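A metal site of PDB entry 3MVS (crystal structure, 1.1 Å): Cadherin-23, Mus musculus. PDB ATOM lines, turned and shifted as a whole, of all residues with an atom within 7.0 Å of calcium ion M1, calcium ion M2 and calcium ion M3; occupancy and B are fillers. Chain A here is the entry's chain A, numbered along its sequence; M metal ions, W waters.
Calcium ion M2 is bound by the side-chain carboxylate (OD1) of Asp 101, at 2.3 Å.
The side-chain carboxylate (OD1) of Asp 137 binds calcium ion M2, 2.3 Å away.
The side-chain carboxylate (OE2) of Glu 21 binds calcium ion M2, 2.3 Å away.
The backbone carbonyl oxygen (O) of Val 102 is bound to calcium ion M2, at 2.4 Å.
OE2 of Glu 73 is bound to calcium ion M2 (2.4 Å).
OD1 of Asp 104 is bound to calcium ion M2 (2.4 Å).
Calcium ion M2 is bound by the side-chain carboxylate (OE1) of Glu 73, at 2.7 Å.
Calcium ion M2 has seven donor atoms within binding distance.
The side-chain carboxylate of Asp 101 is in hydrogen-bond range of the backbone NH of Leu 138 (3.0 Å).
The backbone carbonyl oxygen (O) of Asp 137 lies close to the backbone NH (N) of Gly 142 (3.4 Å).
The side-chain amide nitrogen (ND2) of Asn 105 sits close to the side-chain carboxylate (OE1) of Glu 73, at 3.4 Å.
The side-chain carboxylate (OE1) of Glu 21 lies close to the backbone NH (N) of Arg 72, at 2.9 Å.
N of Glu 21 is in hydrogen-bond range of O of Gly 100 (2.9 Å).
The side-chain carboxylate (OD2) of Asp 71 lies within hydrogen-bond range of the side-chain hydroxyl (OG1) of Thr 74 (2.8 Å).
The backbone NH (N) of Leu 193 sits at hydrogen-bond distance from the side-chain carboxylate (OD1) of Asp 186.
The side-chain amide nitrogen (ND2) of Asn 105 sits close to the side-chain carboxylate (OD1) of Asp 104 (3.1 Å).
Of the 29 residues printed, 4 come within 4 Å of calcium ion M1.
The nearest printed residue that does not touch calcium ion M1 is Arg 72 (4.1 Å).
Calcium ion M1 is bound by water W1 (2.3 Å).
OE1 of Glu 73 is bound to calcium ion M1.
Calcium ion M1 is bound by OD1 of Asp 71 (2.3 Å).
Calcium ion M1 is bound by OE1 of Glu 21, 2.3 Å away.
Calcium ion M1 is bound by water W2, at 2.4 Å.
OD2 of Asp 104 binds calcium ion M1.
Calcium ion M1 has six donor atoms within binding distance.
Slightly farther from calcium ion M1 lies OD1 of Asp 104 (3.1 Å).
Of the 29 residues printed, 6 come within 4 Å of calcium ion M3.
Along chain A the residues within 4 Å of calcium ion M3 span positions 103 to 186.
The nearest printed residue that does not touch calcium ion M3 is Ala 106 (4.5 Å).
Seven residues have an atom within 4 Å of calcium ion M2: Glu 21, Glu 73, Asp 101, Val 102, Asp 104, Asn 105 and Asp 137.
The nearest printed residue that does not touch calcium ion M2 is Asn 103 (4.6 Å).
The backbone carbonyl oxygen (O) of Gly 141 binds calcium ion M3 (2.3 Å).
OD2 of Asp 186 is bound to calcium ion M3 (2.3 Å).
The backbone carbonyl oxygen (O) of Asn 105 is bound to calcium ion M3 (2.3 Å).
Calcium ion M3 is bound by the side-chain amide oxygen (OD1) of Asn 103 (2.4 Å).
OD2 of Asp 135 binds calcium ion M3 (2.4 Å).
OD2 of Asp 137 binds calcium ion M3, at 2.4 Å.
Calcium ion M3 is bound by OD1 of Asp 135, 2.5 Å away.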
ATOM      1  N   GLU A  21      31.424  -0.074  -4.082  1.00  0.00           N
ATOM      2  CA  GLU A  21      30.035  -0.490  -4.198  1.00  0.00           C
ATOM      3  C   GLU A  21      29.328   0.072  -5.433  1.00  0.00           C
ATOM      4  O   GLU A  21      28.260  -0.418  -5.783  1.00  0.00           O
ATOM      5  CB  GLU A  21      29.227  -0.146  -2.944  1.00  0.00           C
ATOM      6  CG  GLU A  21      29.000   1.356  -2.740  1.00  0.00           C
ATOM      7  CD  GLU A  21      28.111   1.699  -1.555  1.00  0.00           C
ATOM      8  OE1 GLU A  21      27.236   0.876  -1.224  1.00  0.00           O
ATOM      9  OE2 GLU A  21      28.260   2.811  -1.003  1.00  0.00           O
ATOM     10  N   LEU A  70      26.923  -4.864  -5.047  1.00  0.00           N
ATOM     11  CA  LEU A  70      27.495  -4.787  -3.712  1.00  0.00           C
ATOM     12  C   LEU A  70      26.847  -3.603  -3.014  1.00  0.00           C
ATOM     13  O   LEU A  70      26.410  -2.663  -3.670  1.00  0.00           O
ATOM     14  CB  LEU A  70      29.001  -4.556  -3.784  1.00  0.00           C
ATOM     15  CG  LEU A  70      29.780  -5.642  -4.515  1.00  0.00           C
ATOM     16  CD1 LEU A  70      31.217  -5.199  -4.673  1.00  0.00           C
ATOM     17  CD2 LEU A  70      29.687  -6.965  -3.792  1.00  0.00           C
ATOM     18  N   ASP A  71      26.742  -3.673  -1.696  1.00  0.00           N
ATOM     19  CA  ASP A  71      26.140  -2.577  -0.954  1.00  0.00           C
ATOM     20  C   ASP A  71      26.875  -2.442   0.350  1.00  0.00           C
ATOM     21  O   ASP A  71      26.709  -3.260   1.245  1.00  0.00           O
ATOM     22  CB  ASP A  71      24.650  -2.818  -0.725  1.00  0.00           C
ATOM     23  CG  ASP A  71      23.990  -1.707   0.069  1.00  0.00           C
ATOM     24  OD1 ASP A  71      24.574  -0.609   0.193  1.00  0.00           O
ATOM     25  OD2 ASP A  71      22.857  -1.923   0.575  1.00  0.00           O
ATOM     26  N   ARG A  72      27.685  -1.395   0.456  1.00  0.00           N
ATOM     27  CA  ARG A  72      28.467  -1.140   1.655  1.00  0.00           C
ATOM     28  C   ARG A  72      27.590  -1.020   2.892  1.00  0.00           C
ATOM     29  O   ARG A  72      27.973  -1.428   3.992  1.00  0.00           O
ATOM     30  CB  ARG A  72      29.311   0.122   1.473  1.00  0.00           C
ATOM     31  CG  ARG A  72      30.569   0.242   2.339  1.00  0.00           C
ATOM     32  CD  ARG A  72      30.340   0.683   3.780  1.00  0.00           C
ATOM     33  NE  ARG A  72      29.333   1.734   3.851  1.00  0.00           N
ATOM     34  CZ  ARG A  72      28.731   2.081   4.993  1.00  0.00           C
ATOM     35  NH1 ARG A  72      29.071   1.475   6.124  1.00  0.00           N
ATOM     36  NH2 ARG A  72      27.811   3.042   5.001  1.00  0.00           N
ATOM     37  N   GLU A  73      26.385  -0.490   2.692  1.00  0.00           N
ATOM     38  CA  GLU A  73      25.419  -0.295   3.794  1.00  0.00           C
ATOM     39  C   GLU A  73      24.788  -1.592   4.304  1.00  0.00           C
ATOM     40  O   GLU A  73      24.138  -1.585   5.359  1.00  0.00           O
ATOM     41  CB  GLU A  73      24.313   0.683   3.373  1.00  0.00           C
ATOM     42  CG  GLU A  73      24.666   2.161   3.407  1.00  0.00           C
ATOM     43  CD  GLU A  73      25.623   2.604   2.302  1.00  0.00           C
ATOM     44  OE1 GLU A  73      25.470   2.253   1.109  1.00  0.00           O
ATOM     45  OE2 GLU A  73      26.551   3.353   2.627  1.00  0.00           O
ATOM     46  N   THR A  74      24.960  -2.691   3.570  1.00  0.00           N
ATOM     47  CA  THR A  74      24.441  -4.007   3.969  1.00  0.00           C
ATOM     48  C   THR A  74      25.565  -4.897   4.476  1.00  0.00           C
ATOM     49  O   THR A  74      25.453  -5.504   5.546  1.00  0.00           O
ATOM     50  CB  THR A  74      23.700  -4.710   2.805  1.00  0.00           C
ATOM     51  OG1 THR A  74      22.564  -3.943   2.418  1.00  0.00           O
ATOM     52  CG2 THR A  74      23.255  -6.113   3.196  1.00  0.00           C
ATOM     53  N   GLY A 100      33.977  -0.833  -0.888  1.00  0.00           N
ATOM     54  CA  GLY A 100      34.252   0.586  -0.687  1.00  0.00           C
ATOM     55  C   GLY A 100      32.969   1.394  -0.718  1.00  0.00           C
ATOM     56  O   GLY A 100      32.094   1.167  -1.548  1.00  0.00           O
ATOM     57  N   ASP A 101      32.865   2.364   0.184  1.00  0.00           N
ATOM     58  CA  ASP A 101      31.675   3.207   0.245  1.00  0.00           C
ATOM     59  C   ASP A 101      31.720   4.272  -0.830  1.00  0.00           C
ATOM     60  O   ASP A 101      32.761   4.863  -1.088  1.00  0.00           O
ATOM     61  CB  ASP A 101      31.577   3.878   1.609  1.00  0.00           C
ATOM     62  CG  ASP A 101      30.248   4.605   1.812  1.00  0.00           C
ATOM     63  OD1 ASP A 101      29.200   3.970   1.649  1.00  0.00           O
ATOM     64  OD2 ASP A 101      30.239   5.805   2.170  1.00  0.00           O
ATOM     65  N   VAL A 102      30.553   4.555  -1.400  1.00  0.00           N
ATOM     66  CA  VAL A 102      30.359   5.808  -2.149  1.00  0.00           C
ATOM     67  C   VAL A 102      29.137   6.505  -1.578  1.00  0.00           C
ATOM     68  O   VAL A 102      28.346   5.907  -0.833  1.00  0.00           O
ATOM     69  CB  VAL A 102      30.214   5.611  -3.691  1.00  0.00           C
ATOM     70  CG1 VAL A 102      31.375   4.812  -4.241  1.00  0.00           C
ATOM     71  CG2 VAL A 102      28.886   4.971  -4.034  1.00  0.00           C
ATOM     72  N   ASN A 103      28.941   7.767  -1.942  1.00  0.00           N
ATOM     73  CA  ASN A 103      27.747   8.468  -1.503  1.00  0.00           C
ATOM     74  C   ASN A 103      26.605   8.086  -2.422  1.00  0.00           C
ATOM     75  O   ASN A 103      26.465   8.646  -3.511  1.00  0.00           O
ATOM     76  CB  ASN A 103      27.937   9.981  -1.531  1.00  0.00           C
ATOM     77  CG  ASN A 103      26.789  10.681  -0.863  1.00  0.00           C
ATOM     78  OD1 ASN A 103      26.387  10.274   0.209  1.00  0.00           O
ATOM     79  ND2 ASN A 103      26.264  11.716  -1.487  1.00  0.00           N
ATOM     80  N   ASP A 104      25.798   7.127  -1.994  1.00  0.00           N
ATOM     81  CA  ASP A 104      24.701   6.611  -2.822  1.00  0.00           C
ATOM     82  C   ASP A 104      23.342   6.613  -2.134  1.00  0.00           C
ATOM     83  O   ASP A 104      22.371   6.070  -2.655  1.00  0.00           O
ATOM     84  CB  ASP A 104      25.033   5.231  -3.430  1.00  0.00           C
ATOM     85  CG  ASP A 104      25.293   4.133  -2.391  1.00  0.00           C
ATOM     86  OD1 ASP A 104      25.489   4.413  -1.191  1.00  0.00           O
ATOM     87  OD2 ASP A 104      25.282   2.935  -2.768  1.00  0.00           O
ATOM     88  N   ASN A 105      23.282   7.262  -0.978  1.00  0.00           N
ATOM     89  CA  ASN A 105      22.010   7.462  -0.274  1.00  0.00           C
ATOM     90  C   ASN A 105      21.764   8.948  -0.103  1.00  0.00           C
ATOM     91  O   ASN A 105      22.658   9.697   0.236  1.00  0.00           O
ATOM     92  CB  ASN A 105      22.011   6.836   1.129  1.00  0.00           C
ATOM     93  CG  ASN A 105      22.077   5.332   1.085  1.00  0.00           C
ATOM     94  OD1 ASN A 105      21.051   4.647   1.170  1.00  0.00           O
ATOM     95  ND2 ASN A 105      23.286   4.797   0.908  1.00  0.00           N
ATOM     96  N   ALA A 106      20.537   9.375  -0.375  1.00  0.00           N
ATOM     97  CA  ALA A 106      20.101  10.708   0.037  1.00  0.00           C
ATOM     98  C   ALA A 106      19.581  10.624   1.469  1.00  0.00           C
ATOM     99  O   ALA A 106      19.283   9.535   1.964  1.00  0.00           O
ATOM    100  CB  ALA A 106      19.002  11.199  -0.908  1.00  0.00           C
ATOM    101  N   PRO A 107      19.429  11.771   2.147  1.00  0.00           N
ATOM    102  CA  PRO A 107      18.892  11.741   3.521  1.00  0.00           C
ATOM    103  C   PRO A 107      17.443  11.245   3.592  1.00  0.00           C
ATOM    104  O   PRO A 107      16.677  11.420   2.649  1.00  0.00           O
ATOM    105  CB  PRO A 107      19.012  13.205   3.974  1.00  0.00           C
ATOM    106  CG  PRO A 107      20.155  13.732   3.148  1.00  0.00           C
ATOM    107  CD  PRO A 107      19.975  13.102   1.804  1.00  0.00           C
ATOM    108  N   ASP A 135      21.373   9.863   7.307  1.00  0.00           N
ATOM    109  CA  ASP A 135      21.958   9.434   6.050  1.00  0.00           C
ATOM    110  C   ASP A 135      23.052   8.415   6.376  1.00  0.00           C
ATOM    111  O   ASP A 135      23.949   8.725   7.162  1.00  0.00           O
ATOM    112  CB  ASP A 135      22.537  10.665   5.350  1.00  0.00           C
ATOM    113  CG  ASP A 135      23.019  10.393   3.944  1.00  0.00           C
ATOM    114  OD1 ASP A 135      23.691   9.368   3.693  1.00  0.00           O
ATOM    115  OD2 ASP A 135      22.783  11.251   3.055  1.00  0.00           O
ATOM    116  N   PRO A 136      23.005   7.206   5.787  1.00  0.00           N
ATOM    117  CA  PRO A 136      23.894   6.115   6.237  1.00  0.00           C
ATOM    118  C   PRO A 136      25.255   6.090   5.565  1.00  0.00           C
ATOM    119  O   PRO A 136      26.090   5.255   5.930  1.00  0.00           O
ATOM    120  CB  PRO A 136      23.121   4.868   5.831  1.00  0.00           C
ATOM    121  CG  PRO A 136      22.435   5.270   4.574  1.00  0.00           C
ATOM    122  CD  PRO A 136      21.979   6.719   4.858  1.00  0.00           C
ATOM    123  N   ASP A 137      25.508   6.940   4.572  1.00  0.00           N
ATOM    124  CA  ASP A 137      26.808   6.947   3.927  1.00  0.00           C
ATOM    125  C   ASP A 137      27.883   7.393   4.893  1.00  0.00           C
ATOM    126  O   ASP A 137      27.589   8.072   5.876  1.00  0.00           O
ATOM    127  CB  ASP A 137      26.809   7.828   2.678  1.00  0.00           C
ATOM    128  CG  ASP A 137      25.876   7.306   1.605  1.00  0.00           C
ATOM    129  OD1 ASP A 137      26.029   6.137   1.191  1.00  0.00           O
ATOM    130  OD2 ASP A 137      24.971   8.057   1.200  1.00  0.00           O
ATOM    131  N   LEU A 138      29.119   7.034   4.618  1.00  0.00           N
ATOM    132  CA  LEU A 138      30.201   7.349   5.519  1.00  0.00           C
ATOM    133  C   LEU A 138      30.701   8.766   5.329  1.00  0.00           C
ATOM    134  O   LEU A 138      30.542   9.352   4.241  1.00  0.00           O
ATOM    135  CB  LEU A 138      31.357   6.350   5.350  1.00  0.00           C
ATOM    136  CG  LEU A 138      30.980   4.899   5.592  1.00  0.00           C
ATOM    137  CD1 LEU A 138      32.199   3.991   5.461  1.00  0.00           C
ATOM    138  CD2 LEU A 138      30.334   4.716   6.980  1.00  0.00           C
ATOM    139  N   ALA A 140      31.522  12.643   5.021  1.00  0.00           N
ATOM    140  CA  ALA A 140      30.762  13.828   4.632  1.00  0.00           C
ATOM    141  C   ALA A 140      29.458  13.474   3.929  1.00  0.00           C
ATOM    142  O   ALA A 140      28.476  14.196   4.045  1.00  0.00           O
ATOM    143  CB  ALA A 140      31.608  14.742   3.766  1.00  0.00           C
ATOM    144  N   GLY A 141      29.443  12.328   3.242  1.00  0.00           N
ATOM    145  CA  GLY A 141      28.226  11.864   2.609  1.00  0.00           C
ATOM    146  C   GLY A 141      27.118  11.468   3.559  1.00  0.00           C
ATOM    147  O   GLY A 141      25.983  11.277   3.111  1.00  0.00           O
ATOM    148  N   GLY A 142      27.423  11.333   4.859  1.00  0.00           N
ATOM    149  CA  GLY A 142      26.415  11.029   5.871  1.00  0.00           C
ATOM    150  C   GLY A 142      26.032  12.225   6.725  1.00  0.00           C
ATOM    151  O   GLY A 142      25.200  12.097   7.615  1.00  0.00           O
ATOM    152  N   SER A 143      26.665  13.370   6.443  1.00  0.00           N
ATOM    153  CA  SER A 143      26.409  14.603   7.178  1.00  0.00           C
ATOM    154  C   SER A 143      25.359  15.431   6.451  1.00  0.00           C
ATOM    155  O   SER A 143      25.499  15.709   5.268  1.00  0.00           O
ATOM    156  CB  SER A 143      27.705  15.411   7.309  1.00  0.00           C
ATOM    157  OG  SER A 143      27.480  16.627   7.979  1.00  0.00           O
ATOM    158  N   VAL A 144      24.325  15.825   7.178  1.00  0.00           N
ATOM    159  CA  VAL A 144      23.139  16.465   6.590  1.00  0.00           C
ATOM    160  C   VAL A 144      23.054  17.934   6.981  1.00  0.00           C
ATOM    161  O   VAL A 144      23.245  18.290   8.154  1.00  0.00           O
ATOM    162  CB  VAL A 144      21.868  15.727   7.102  1.00  0.00           C
ATOM    163  CG1 VAL A 144      20.599  16.392   6.544  1.00  0.00           C
ATOM    164  CG2 VAL A 144      21.907  14.253   6.708  1.00  0.00           C
ATOM    165  N   ASP A 186      23.194  16.116   1.811  1.00  0.00           N
ATOM    166  CA  ASP A 186      24.420  15.657   2.419  1.00  0.00           C
ATOM    167  C   ASP A 186      25.615  16.453   1.923  1.00  0.00           C
ATOM    168  O   ASP A 186      25.506  17.300   1.043  1.00  0.00           O
ATOM    169  CB  ASP A 186      24.563  14.122   2.300  1.00  0.00           C
ATOM    170  CG  ASP A 186      24.787  13.654   0.881  1.00  0.00           C
ATOM    171  OD1 ASP A 186      25.383  14.401   0.082  1.00  0.00           O
ATOM    172  OD2 ASP A 186      24.397  12.506   0.558  1.00  0.00           O
ATOM    173  N   GLN A 187      26.777  16.201   2.512  1.00  0.00           N
ATOM    174  CA  GLN A 187      27.932  17.074   2.316  1.00  0.00           C
ATOM    175  C   GLN A 187      29.055  16.427   1.515  1.00  0.00           C
ATOM    176  O   GLN A 187      30.205  16.881   1.559  1.00  0.00           O
ATOM    177  CB  GLN A 187      28.421  17.614   3.663  1.00  0.00           C
ATOM    178  CG  GLN A 187      27.346  18.422   4.393  1.00  0.00           C
ATOM    179  CD  GLN A 187      26.861  19.586   3.567  1.00  0.00           C
ATOM    180  OE1 GLN A 187      25.698  19.645   3.171  1.00  0.00           O
ATOM    181  NE2 GLN A 187      27.758  20.524   3.299  1.00  0.00           N
ATOM    182  N   ASP A 188      28.738  15.376   0.767  1.00  0.00           N
ATOM    183  CA  ASP A 188      29.751  14.772  -0.098  1.00  0.00           C
ATOM    184  C   ASP A 188      30.308  15.830  -1.054  1.00  0.00           C
ATOM    185  O   ASP A 188      29.559  16.618  -1.629  1.00  0.00           O
ATOM    186  CB  ASP A 188      29.167  13.617  -0.908  1.00  0.00           C
ATOM    187  CG  ASP A 188      30.240  12.861  -1.649  1.00  0.00           C
ATOM    188  OD1 ASP A 188      30.902  12.011  -1.033  1.00  0.00           O
ATOM    189  OD2 ASP A 188      30.442  13.142  -2.847  1.00  0.00           O
ATOM    190  N   ARG A 191      29.640  14.393  -5.140  1.00  0.00           N
ATOM    191  CA  ARG A 191      28.283  14.094  -5.575  1.00  0.00           C
ATOM    192  C   ARG A 191      27.276  14.144  -4.415  1.00  0.00           C
ATOM    193  O   ARG A 191      26.747  13.104  -3.991  1.00  0.00           O
ATOM    194  CB  ARG A 191      28.227  12.760  -6.304  1.00  0.00           C
ATOM    195  CG  ARG A 191      27.340  12.800  -7.529  1.00  0.00           C
ATOM    196  N   PRO A 192      26.995  15.351  -3.924  1.00  0.00           N
ATOM    197  CA  PRO A 192      26.008  15.484  -2.859  1.00  0.00           C
ATOM    198  C   PRO A 192      24.600  15.080  -3.315  1.00  0.00           C
ATOM    199  O   PRO A 192      24.257  15.271  -4.495  1.00  0.00           O
ATOM    200  CB  PRO A 192      26.075  16.959  -2.484  1.00  0.00           C
ATOM    201  CG  PRO A 192      26.591  17.643  -3.712  1.00  0.00           C
ATOM    202  CD  PRO A 192      27.537  16.664  -4.317  1.00  0.00           C
ATOM    203  N   LEU A 193      23.816  14.544  -2.383  1.00  0.00           N
ATOM    204  CA  LEU A 193      22.470  14.084  -2.653  1.00  0.00           C
ATOM    205  C   LEU A 193      21.467  14.769  -1.747  1.00  0.00           C
ATOM    206  O   LEU A 193      21.770  15.033  -0.580  1.00  0.00           O
ATOM    207  CB  LEU A 193      22.398  12.575  -2.482  1.00  0.00           C
ATOM    208  CG  LEU A 193      23.236  11.777  -3.486  1.00  0.00           C
ATOM    209  CD1 LEU A 193      23.176  10.295  -3.117  1.00  0.00           C
ATOM    210  CD2 LEU A 193      22.763  11.952  -4.914  1.00  0.00           C
HETATM  211 CA    CA M   1      24.958   1.379  -0.988  1.00  0.00          CA
HETATM  212 CA    CA M   2      27.226   4.273   0.499  1.00  0.00          CA
HETATM  213 CA    CA M   3      24.464  10.391   1.567  1.00  0.00          CA
HETATM  214  O   HOH W   1      24.103   0.106  -2.734  1.00  0.00           O
HETATM  215  O   HOH W   2      22.770   2.124  -0.549  1.00  0.00           O
